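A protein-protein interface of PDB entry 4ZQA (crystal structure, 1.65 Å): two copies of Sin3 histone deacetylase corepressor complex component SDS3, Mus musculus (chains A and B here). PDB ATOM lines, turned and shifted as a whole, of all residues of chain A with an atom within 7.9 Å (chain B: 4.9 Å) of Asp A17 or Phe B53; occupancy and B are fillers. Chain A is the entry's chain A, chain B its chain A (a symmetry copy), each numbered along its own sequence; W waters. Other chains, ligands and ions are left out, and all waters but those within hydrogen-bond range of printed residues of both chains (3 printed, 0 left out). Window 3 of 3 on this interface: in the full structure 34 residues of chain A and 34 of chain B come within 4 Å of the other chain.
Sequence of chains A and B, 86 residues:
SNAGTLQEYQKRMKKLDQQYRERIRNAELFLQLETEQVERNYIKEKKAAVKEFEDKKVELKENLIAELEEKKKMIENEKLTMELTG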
ATOM      1  N   LYS A  11      11.848 -28.024 -29.321  1.00  0.00           N
ATOM      2  CA  LYS A  11      11.630 -29.459 -29.052  1.00  0.00           C
ATOM      3  C   LYS A  11      11.100 -29.617 -27.635  1.00  0.00           C
ATOM      4  O   LYS A  11      10.127 -30.330 -27.379  1.00  0.00           O
ATOM      5  CB  LYS A  11      12.952 -30.244 -29.204  1.00  0.00           C
ATOM      6  CG  LYS A  11      12.821 -31.762 -29.135  1.00  0.00           C
ATOM      7  CD  LYS A  11      14.151 -32.452 -28.788  1.00  0.00           C
ATOM      8  CE  LYS A  11      15.341 -31.834 -29.504  1.00  0.00           C
ATOM      9  NZ  LYS A  11      16.615 -32.583 -29.265  1.00  0.00           N
ATOM     10  N   ARG A  12      11.754 -28.955 -26.702  1.00  0.00           N
ATOM     11  CA  ARG A  12      11.408 -29.113 -25.304  1.00  0.00           C
ATOM     12  C   ARG A  12      10.045 -28.497 -24.995  1.00  0.00           C
ATOM     13  O   ARG A  12       9.294 -29.028 -24.183  1.00  0.00           O
ATOM     14  CB  ARG A  12      12.502 -28.518 -24.407  1.00  0.00           C
ATOM     15  CG  ARG A  12      13.784 -29.306 -24.445  1.00  0.00           C
ATOM     16  CD  ARG A  12      14.880 -28.625 -23.654  1.00  0.00           C
ATOM     17  NE  ARG A  12      16.058 -29.485 -23.544  1.00  0.00           N
ATOM     18  CZ  ARG A  12      17.279 -29.079 -23.207  1.00  0.00           C
ATOM     19  NH1 ARG A  12      17.539 -27.799 -22.971  1.00  0.00           N
ATOM     20  NH2 ARG A  12      18.253 -29.965 -23.141  1.00  0.00           N
ATOM     21  N   MET A  13       9.732 -27.379 -25.625  1.00  0.00           N
ATOM     22  CA  MET A  13       8.398 -26.764 -25.464  1.00  0.00           C
ATOM     23  C   MET A  13       7.294 -27.717 -25.925  1.00  0.00           C
ATOM     24  O   MET A  13       6.313 -27.896 -25.227  1.00  0.00           O
ATOM     25  CB  MET A  13       8.318 -25.457 -26.246  1.00  0.00           C
ATOM     26  CG  MET A  13       9.127 -24.361 -25.570  1.00  0.00           C
ATOM     27  SD  MET A  13       8.242 -23.774 -24.111  1.00  0.00           S
ATOM     28  CE  MET A  13       6.913 -22.793 -24.863  1.00  0.00           C
ATOM     29  N   LYS A  14       7.467 -28.320 -27.106  1.00  0.00           N
ATOM     30  CA  LYS A  14       6.533 -29.337 -27.620  1.00  0.00           C
ATOM     31  C   LYS A  14       6.362 -30.531 -26.635  1.00  0.00           C
ATOM     32  O   LYS A  14       5.228 -31.011 -26.438  1.00  0.00           O
ATOM     33  CB  LYS A  14       6.982 -29.801 -29.029  1.00  0.00           C
ATOM     34  CG  LYS A  14       6.083 -30.827 -29.666  1.00  0.00           C
ATOM     35  CD  LYS A  14       6.472 -31.138 -31.116  1.00  0.00           C
ATOM     36  CE  LYS A  14       5.959 -32.515 -31.550  1.00  0.00           C
ATOM     37  NZ  LYS A  14       4.570 -32.810 -31.064  1.00  0.00           N
ATOM     38  N   LYS A  15       7.462 -30.992 -26.020  1.00  0.00           N
ATOM     39  CA  LYS A  15       7.389 -32.073 -25.025  1.00  0.00           C
ATOM     40  C   LYS A  15       6.604 -31.631 -23.789  1.00  0.00           C
ATOM     41  O   LYS A  15       5.787 -32.398 -23.266  1.00  0.00           O
ATOM     42  CB  LYS A  15       8.787 -32.538 -24.604  1.00  0.00           C
ATOM     43  CG  LYS A  15       8.821 -33.780 -23.705  1.00  0.00           C
ATOM     44  CD  LYS A  15       8.032 -34.947 -24.295  1.00  0.00           C
ATOM     45  CE  LYS A  15       8.242 -36.249 -23.541  1.00  0.00           C
ATOM     46  NZ  LYS A  15       7.000 -37.090 -23.520  1.00  0.00           N
ATOM     47  N   LEU A  16       6.824 -30.390 -23.331  1.00  0.00           N
ATOM     48  CA  LEU A  16       6.041 -29.884 -22.200  1.00  0.00           C
ATOM     49  C   LEU A  16       4.551 -29.896 -22.475  1.00  0.00           C
ATOM     50  O   LEU A  16       3.763 -30.273 -21.606  1.00  0.00           O
ATOM     51  CB  LEU A  16       6.481 -28.483 -21.790  1.00  0.00           C
ATOM     52  CG  LEU A  16       7.815 -28.327 -21.060  1.00  0.00           C
ATOM     53  CD1 LEU A  16       7.946 -26.824 -20.717  1.00  0.00           C
ATOM     54  CD2 LEU A  16       7.966 -29.214 -19.820  1.00  0.00           C
ATOM     55  N   ASP A  17       4.183 -29.503 -23.685  1.00  0.00           N
ATOM     56  CA  ASP A  17       2.817 -29.482 -24.105  1.00  0.00           C
ATOM     57  C   ASP A  17       2.222 -30.921 -24.176  1.00  0.00           C
ATOM     58  O   ASP A  17       1.120 -31.171 -23.644  1.00  0.00           O
ATOM     59  CB  ASP A  17       2.665 -28.748 -25.436  1.00  0.00           C
ATOM     60  CG  ASP A  17       1.224 -28.722 -25.916  1.00  0.00           C
ATOM     61  OD1 ASP A  17       0.469 -27.802 -25.536  1.00  0.00           O
ATOM     62  OD2 ASP A  17       0.837 -29.647 -26.666  1.00  0.00           O
ATOM     63  N   GLN A  18       2.966 -31.854 -24.801  1.00  0.00           N
ATOM     64  CA  GLN A  18       2.603 -33.264 -24.826  1.00  0.00           C
ATOM     65  C   GLN A  18       2.332 -33.805 -23.409  1.00  0.00           C
ATOM     66  O   GLN A  18       1.327 -34.485 -23.178  1.00  0.00           O
ATOM     67  CB  GLN A  18       3.734 -34.029 -25.551  1.00  0.00           C
ATOM     68  CG  GLN A  18       3.658 -35.522 -25.571  1.00  0.00           C
ATOM     69  CD  GLN A  18       4.700 -36.107 -26.505  1.00  0.00           C
ATOM     70  OE1 GLN A  18       5.749 -35.468 -26.783  1.00  0.00           O
ATOM     71  NE2 GLN A  18       4.406 -37.288 -27.040  1.00  0.00           N
ATOM     72  N   GLN A  19       3.198 -33.465 -22.460  1.00  0.00           N
ATOM     73  CA  GLN A  19       3.099 -33.928 -21.084  1.00  0.00           C
ATOM     74  C   GLN A  19       1.889 -33.314 -20.346  1.00  0.00           C
ATOM     75  O   GLN A  19       1.183 -33.991 -19.574  1.00  0.00           O
ATOM     76  CB  GLN A  19       4.397 -33.635 -20.331  1.00  0.00           C
ATOM     77  CG  GLN A  19       5.580 -34.438 -20.842  1.00  0.00           C
ATOM     78  CD  GLN A  19       6.948 -34.059 -20.298  1.00  0.00           C
ATOM     79  OE1 GLN A  19       7.888 -34.820 -20.485  1.00  0.00           O
ATOM     80  NE2 GLN A  19       7.081 -32.917 -19.647  1.00  0.00           N
ATOM     81  N   TYR A  20       1.651 -32.040 -20.606  1.00  0.00           N
ATOM     82  CA  TYR A  20       0.453 -31.395 -20.095  1.00  0.00           C
ATOM     83  C   TYR A  20      -0.834 -32.093 -20.594  1.00  0.00           C
ATOM     84  O   TYR A  20      -1.699 -32.483 -19.800  1.00  0.00           O
ATOM     85  CB  TYR A  20       0.456 -29.910 -20.490  1.00  0.00           C
ATOM     86  CG  TYR A  20      -0.862 -29.296 -20.269  1.00  0.00           C
ATOM     87  CD1 TYR A  20      -1.328 -29.099 -18.961  1.00  0.00           C
ATOM     88  CD2 TYR A  20      -1.710 -28.960 -21.344  1.00  0.00           C
ATOM     89  CE1 TYR A  20      -2.576 -28.508 -18.734  1.00  0.00           C
ATOM     90  CE2 TYR A  20      -2.977 -28.391 -21.107  1.00  0.00           C
ATOM     91  CZ  TYR A  20      -3.395 -28.198 -19.772  1.00  0.00           C
ATOM     92  OH  TYR A  20      -4.621 -27.683 -19.432  1.00  0.00           O
ATOM     93  N   ARG A  21      -0.919 -32.343 -21.897  1.00  0.00           N
ATOM     94  CA  ARG A  21      -2.109 -32.938 -22.503  1.00  0.00           C
ATOM     95  C   ARG A  21      -2.292 -34.362 -21.955  1.00  0.00           C
ATOM     96  O   ARG A  21      -3.410 -34.776 -21.683  1.00  0.00           O
ATOM     97  CB  ARG A  21      -2.018 -32.971 -24.035  1.00  0.00           C
ATOM     98  CG  ARG A  21      -2.359 -31.648 -24.747  1.00  0.00           C
ATOM     99  CD  ARG A  21      -2.222 -31.798 -26.265  1.00  0.00           C
ATOM    100  NE  ARG A  21      -0.821 -31.969 -26.609  1.00  0.00           N
ATOM    101  CZ  ARG A  21      -0.309 -32.000 -27.839  1.00  0.00           C
ATOM    102  NH1 ARG A  21      -1.085 -31.882 -28.919  1.00  0.00           N
ATOM    103  NH2 ARG A  21       1.006 -32.153 -27.973  1.00  0.00           N
ATOM    104  N   GLU A  22      -1.182 -35.087 -21.784  1.00  0.00           N
ATOM    105  CA  GLU A  22      -1.252 -36.449 -21.227  1.00  0.00           C
ATOM    106  C   GLU A  22      -1.701 -36.423 -19.759  1.00  0.00           C
ATOM    107  O   GLU A  22      -2.498 -37.268 -19.317  1.00  0.00           O
ATOM    108  CB  GLU A  22       0.084 -37.155 -21.372  1.00  0.00           C
ATOM    109  CG  GLU A  22       0.074 -38.584 -20.824  1.00  0.00           C
ATOM    110  CD  GLU A  22      -0.737 -39.656 -21.631  1.00  0.00           C
ATOM    111  OE1 GLU A  22      -1.451 -39.426 -22.679  1.00  0.00           O
ATOM    112  OE2 GLU A  22      -0.633 -40.830 -21.193  1.00  0.00           O
ATOM    113  N   ARG A  23      -1.209 -35.451 -19.003  1.00  0.00           N
ATOM    114  CA  ARG A  23      -1.631 -35.321 -17.609  1.00  0.00           C
ATOM    115  C   ARG A  23      -3.165 -35.057 -17.513  1.00  0.00           C
ATOM    116  O   ARG A  23      -3.854 -35.652 -16.676  1.00  0.00           O
ATOM    117  CB  ARG A  23      -0.819 -34.249 -16.898  1.00  0.00           C
ATOM    118  CG  ARG A  23      -1.077 -34.165 -15.401  1.00  0.00           C
ATOM    119  CD  ARG A  23      -0.073 -33.310 -14.631  1.00  0.00           C
ATOM    120  NE  ARG A  23      -0.513 -33.211 -13.241  1.00  0.00           N
ATOM    121  CZ  ARG A  23       0.135 -32.602 -12.256  1.00  0.00           C
ATOM    122  NH1 ARG A  23       1.255 -31.950 -12.493  1.00  0.00           N
ATOM    123  NH2 ARG A  23      -0.363 -32.626 -11.022  1.00  0.00           N
ATOM    124  N   ILE A  24      -3.688 -34.201 -18.380  1.00  0.00           N
ATOM    125  CA  ILE A  24      -5.149 -33.911 -18.433  1.00  0.00           C
ATOM    126  C   ILE A  24      -5.936 -35.152 -18.842  1.00  0.00           C
ATOM    127  O   ILE A  24      -6.943 -35.479 -18.217  1.00  0.00           O
ATOM    128  CB  ILE A  24      -5.467 -32.732 -19.409  1.00  0.00           C
ATOM    129  CG1 ILE A  24      -4.780 -31.446 -18.901  1.00  0.00           C
ATOM    130  CG2 ILE A  24      -6.977 -32.569 -19.649  1.00  0.00           C
ATOM    131  CD1 ILE A  24      -5.073 -31.052 -17.448  1.00  0.00           C
ATOM    132  N   ARG A  25      -5.468 -35.845 -19.887  1.00  0.00           N
ATOM    133  CA  ARG A  25      -6.060 -37.113 -20.324  1.00  0.00           C
ATOM    134  C   ARG A  25      -6.120 -38.145 -19.190  1.00  0.00           C
ATOM    135  O   ARG A  25      -7.166 -38.804 -18.964  1.00  0.00           O
ATOM    136  CB  ARG A  25      -5.197 -37.641 -21.476  1.00  0.00           C
ATOM    137  CG  ARG A  25      -5.765 -38.728 -22.311  1.00  0.00           C
ATOM    138  CD  ARG A  25      -4.859 -38.955 -23.521  1.00  0.00           C
ATOM    139  NE  ARG A  25      -4.829 -37.814 -24.435  1.00  0.00           N
ATOM    140  CZ  ARG A  25      -3.747 -37.096 -24.775  1.00  0.00           C
ATOM    141  NH1 ARG A  25      -2.551 -37.346 -24.271  1.00  0.00           N
ATOM    142  NH2 ARG A  25      -3.870 -36.074 -25.624  1.00  0.00           N
ATOM    143  N   ALA B  49      -2.005 -29.409 -13.114  1.00  0.00           N
ATOM    144  CA  ALA B  49      -1.413 -29.675 -14.456  1.00  0.00           C
ATOM    145  C   ALA B  49      -1.170 -28.358 -15.186  1.00  0.00           C
ATOM    146  O   ALA B  49      -0.095 -28.154 -15.750  1.00  0.00           O
ATOM    147  CB  ALA B  49      -2.322 -30.549 -15.300  1.00  0.00           C
ATOM    148  N   VAL B  50      -2.154 -27.449 -15.149  1.00  0.00           N
ATOM    149  CA  VAL B  50      -1.988 -26.120 -15.789  1.00  0.00           C
ATOM    150  C   VAL B  50      -0.831 -25.352 -15.139  1.00  0.00           C
ATOM    151  O   VAL B  50       0.006 -24.760 -15.850  1.00  0.00           O
ATOM    152  CB  VAL B  50      -3.295 -25.262 -15.748  1.00  0.00           C
ATOM    153  CG1 VAL B  50      -3.068 -23.809 -16.248  1.00  0.00           C
ATOM    154  CG2 VAL B  50      -4.390 -25.921 -16.557  1.00  0.00           C
ATOM    155  N   LYS B  51      -0.763 -25.381 -13.800  1.00  0.00           N
ATOM    156  CA  LYS B  51       0.297 -24.689 -13.042  1.00  0.00           C
ATOM    157  C   LYS B  51       1.693 -25.251 -13.353  1.00  0.00           C
ATOM    158  O   LYS B  51       2.672 -24.477 -13.544  1.00  0.00           O
ATOM    159  CB  LYS B  51       0.045 -24.747 -11.529  1.00  0.00           C
ATOM    160  CG  LYS B  51       1.089 -24.039 -10.678  1.00  0.00           C
ATOM    161  CD  LYS B  51       0.955 -24.402  -9.204  1.00  0.00           C
ATOM    162  CE  LYS B  51       1.815 -23.521  -8.307  1.00  0.00           C
ATOM    163  NZ  LYS B  51       3.293 -23.499  -8.520  1.00  0.00           N
ATOM    164  N   GLU B  52       1.793 -26.565 -13.370  1.00  0.00           N
ATOM    165  CA  GLU B  52       3.019 -27.236 -13.772  1.00  0.00           C
ATOM    166  C   GLU B  52       3.459 -26.818 -15.169  1.00  0.00           C
ATOM    167  O   GLU B  52       4.645 -26.493 -15.353  1.00  0.00           O
ATOM    168  CB  GLU B  52       2.870 -28.789 -13.710  1.00  0.00           C
ATOM    169  CG  GLU B  52       4.070 -29.536 -14.278  1.00  0.00           C
ATOM    170  CD  GLU B  52       3.900 -31.063 -14.289  1.00  0.00           C
ATOM    171  OE1 GLU B  52       2.892 -31.571 -14.843  1.00  0.00           O
ATOM    172  OE2 GLU B  52       4.792 -31.762 -13.757  1.00  0.00           O
ATOM    173  N   PHE B  53       2.534 -26.836 -16.130  1.00  0.00           N
ATOM    174  CA  PHE B  53       2.820 -26.437 -17.523  1.00  0.00           C
ATOM    175  C   PHE B  53       3.385 -25.035 -17.547  1.00  0.00           C
ATOM    176  O   PHE B  53       4.448 -24.788 -18.126  1.00  0.00           O
ATOM    177  CB  PHE B  53       1.543 -26.538 -18.371  1.00  0.00           C
ATOM    178  CG  PHE B  53       1.733 -26.345 -19.874  1.00  0.00           C
ATOM    179  CD1 PHE B  53       2.918 -26.684 -20.528  1.00  0.00           C
ATOM    180  CD2 PHE B  53       0.683 -25.887 -20.639  1.00  0.00           C
ATOM    181  CE1 PHE B  53       3.035 -26.525 -21.893  1.00  0.00           C
ATOM    182  CE2 PHE B  53       0.790 -25.730 -22.002  1.00  0.00           C
ATOM    183  CZ  PHE B  53       1.978 -26.051 -22.641  1.00  0.00           C
ATOM    184  N   GLU B  54       2.679 -24.122 -16.871  1.00  0.00           N
ATOM    185  CA  GLU B  54       3.050 -22.713 -16.877  1.00  0.00           C
ATOM    186  C   GLU B  54       4.390 -22.494 -16.188  1.00  0.00           C
ATOM    187  O   GLU B  54       5.219 -21.740 -16.696  1.00  0.00           O
ATOM    188  CB  GLU B  54       1.937 -21.893 -16.221  1.00  0.00           C
ATOM    189  CG  GLU B  54       0.754 -21.765 -17.177  1.00  0.00           C
ATOM    190  CD  GLU B  54      -0.441 -21.048 -16.594  1.00  0.00           C
ATOM    191  OE1 GLU B  54      -0.463 -20.750 -15.363  1.00  0.00           O
ATOM    192  OE2 GLU B  54      -1.373 -20.799 -17.393  1.00  0.00           O
ATOM    193  N   ASP B  55       4.616 -23.163 -15.054  1.00  0.00           N
ATOM    194  CA  ASP B  55       5.860 -23.040 -14.301  1.00  0.00           C
ATOM    195  C   ASP B  55       7.044 -23.554 -15.131  1.00  0.00           C
ATOM    196  O   ASP B  55       8.086 -22.900 -15.210  1.00  0.00           O
ATOM    197  CB  ASP B  55       5.789 -23.805 -12.975  1.00  0.00           C
ATOM    198  CG  ASP B  55       4.875 -23.142 -11.940  1.00  0.00           C
ATOM    199  OD1 ASP B  55       4.430 -21.979 -12.153  1.00  0.00           O
ATOM    200  OD2 ASP B  55       4.610 -23.808 -10.884  1.00  0.00           O
ATOM    201  N   LYS B  56       6.862 -24.715 -15.756  1.00  0.00           N
ATOM    202  CA  LYS B  56       7.930 -25.318 -16.588  1.00  0.00           C
ATOM    203  C   LYS B  56       8.252 -24.481 -17.804  1.00  0.00           C
ATOM    204  O   LYS B  56       9.403 -24.402 -18.226  1.00  0.00           O
ATOM    205  CB  LYS B  56       7.593 -26.762 -16.980  1.00  0.00           C
ATOM    206  CG  LYS B  56       7.799 -27.683 -15.808  1.00  0.00           C
ATOM    207  CD  LYS B  56       7.616 -29.147 -16.209  1.00  0.00           C
ATOM    208  CE  LYS B  56       7.733 -30.066 -15.009  1.00  0.00           C
ATOM    209  NZ  LYS B  56       7.755 -31.476 -15.471  1.00  0.00           N
ATOM    210  N   LYS B  57       7.234 -23.851 -18.373  1.00  0.00           N
ATOM    211  CA  LYS B  57       7.449 -22.950 -19.515  1.00  0.00           C
ATOM    212  C   LYS B  57       8.237 -21.723 -19.122  1.00  0.00           C
ATOM    213  O   LYS B  57       9.114 -21.302 -19.868  1.00  0.00           O
ATOM    214  CB  LYS B  57       6.149 -22.552 -20.187  1.00  0.00           C
ATOM    215  CG  LYS B  57       5.572 -23.601 -21.132  1.00  0.00           C
ATOM    216  CD  LYS B  57       4.413 -23.070 -21.891  1.00  0.00           C
ATOM    217  CE  LYS B  57       3.226 -22.795 -20.983  1.00  0.00           C
ATOM    218  NZ  LYS B  57       2.061 -22.290 -21.761  1.00  0.00           N
HETATM  219  O   HOH W   1       9.695 -31.890 -18.110  1.00  0.00           O
HETATM  220  O   HOH W   2       5.483 -31.748 -17.665  1.00  0.00           O
HETATM  221  O   HOH W   3       8.591 -21.198 -22.418  1.00  0.00           O
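OE1 of Glu B52 lies within salt-bridge range of NH1 of Arg A23, 2.9 Å away.
OD2 of Asp A17 lies within salt-bridge range of NH2 of Arg A21 (2.8 Å). The side-chain carboxylate (OE2) of Glu B52 lies within salt-bridge range of the side-chain amino group (NZ) of Lys B56 (3.4 Å).
Among the printed residues, merely in contact across the chains: Met A13 with Lys B57 (3.9 Å), Leu A16 with Phe B53 (3.7 Å), Leu A16 with Lys B56 (3.6 Å), Leu A16 with Lys B57 (3.9 Å), Asp A17 with Phe B53 (3.7 Å), Tyr A20 with Ala B49 (3.6 Å), Tyr A20 with Val B50 (3.4 Å), Tyr A20 with Phe B53 (3.8 Å), Arg A23 with Ala B49 (3.6 Å) and Ile A24 with Ala B49 (3.5 Å).
Of the printed residues of chain B, Asp A17 touches Phe B53. Printed residues of chain A within 4 Å of Glu B52: Arg A23. Of the printed residues of chain B, Tyr A20 touches Ala B49 (3.6 Å), Val B50 (3.4 Å) and Phe B53 (3.8 Å). Of the printed residues of chain B, Leu A16 touches Phe B53 (3.7 Å), Lys B56 (3.6 Å) and Lys B57 (3.9 Å). Of the printed residues of chain A, Ala B49 touches Tyr A20 (3.6 Å), Arg A23 (3.6 Å) and Ile A24 (3.5 Å). Lys A15 touches none of the printed residues of chain B. Lys A11 touches none of the printed residues of chain B. The nearest printed residue of chain B that does not touch Asp A17 is Lys B57 (6.6 Å). The nearest residue of chain A that does not touch Phe B53 is Met A13 (4.9 Å).
Of the 9 printed residues of chain B, 6 touch a printed residue of chain A. Printed residues of chain B that touch a printed residue of chain A: Ala B49, Val B50, Glu B52, Phe B53, Lys B56 and Lys B57. Hydrophobic or aromatic side chains of chain B that line the printed part of chain A: Ala B49, Val B50 and Phe B53. Hydrophobic or aromatic side chains of chain A that line the printed part of chain B: Met A13, Leu A16, Tyr A20 and Ile A24. Among the printed residues, Asp or Glu carboxylates within 4 Å of a Lys or Arg side-chain nitrogen of the other chain: Arg A23 with Glu B52.
No position is printed for both chains. Of the 11 pairs that touch across the chains among the printed residues, none has its exchanged pair printed and touching as well.
Water W3 lies within hydrogen-bond range of O of Lys B57 (2.6 Å) and SD of Met A13 (3.1 Å). Water W2 bridges NE2 of Gln A19 and NZ of Lys B56. Water W1 lies within hydrogen-bond range of the side-chain amide nitrogen of Gln A19 and the side-chain amino group of Lys B56.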
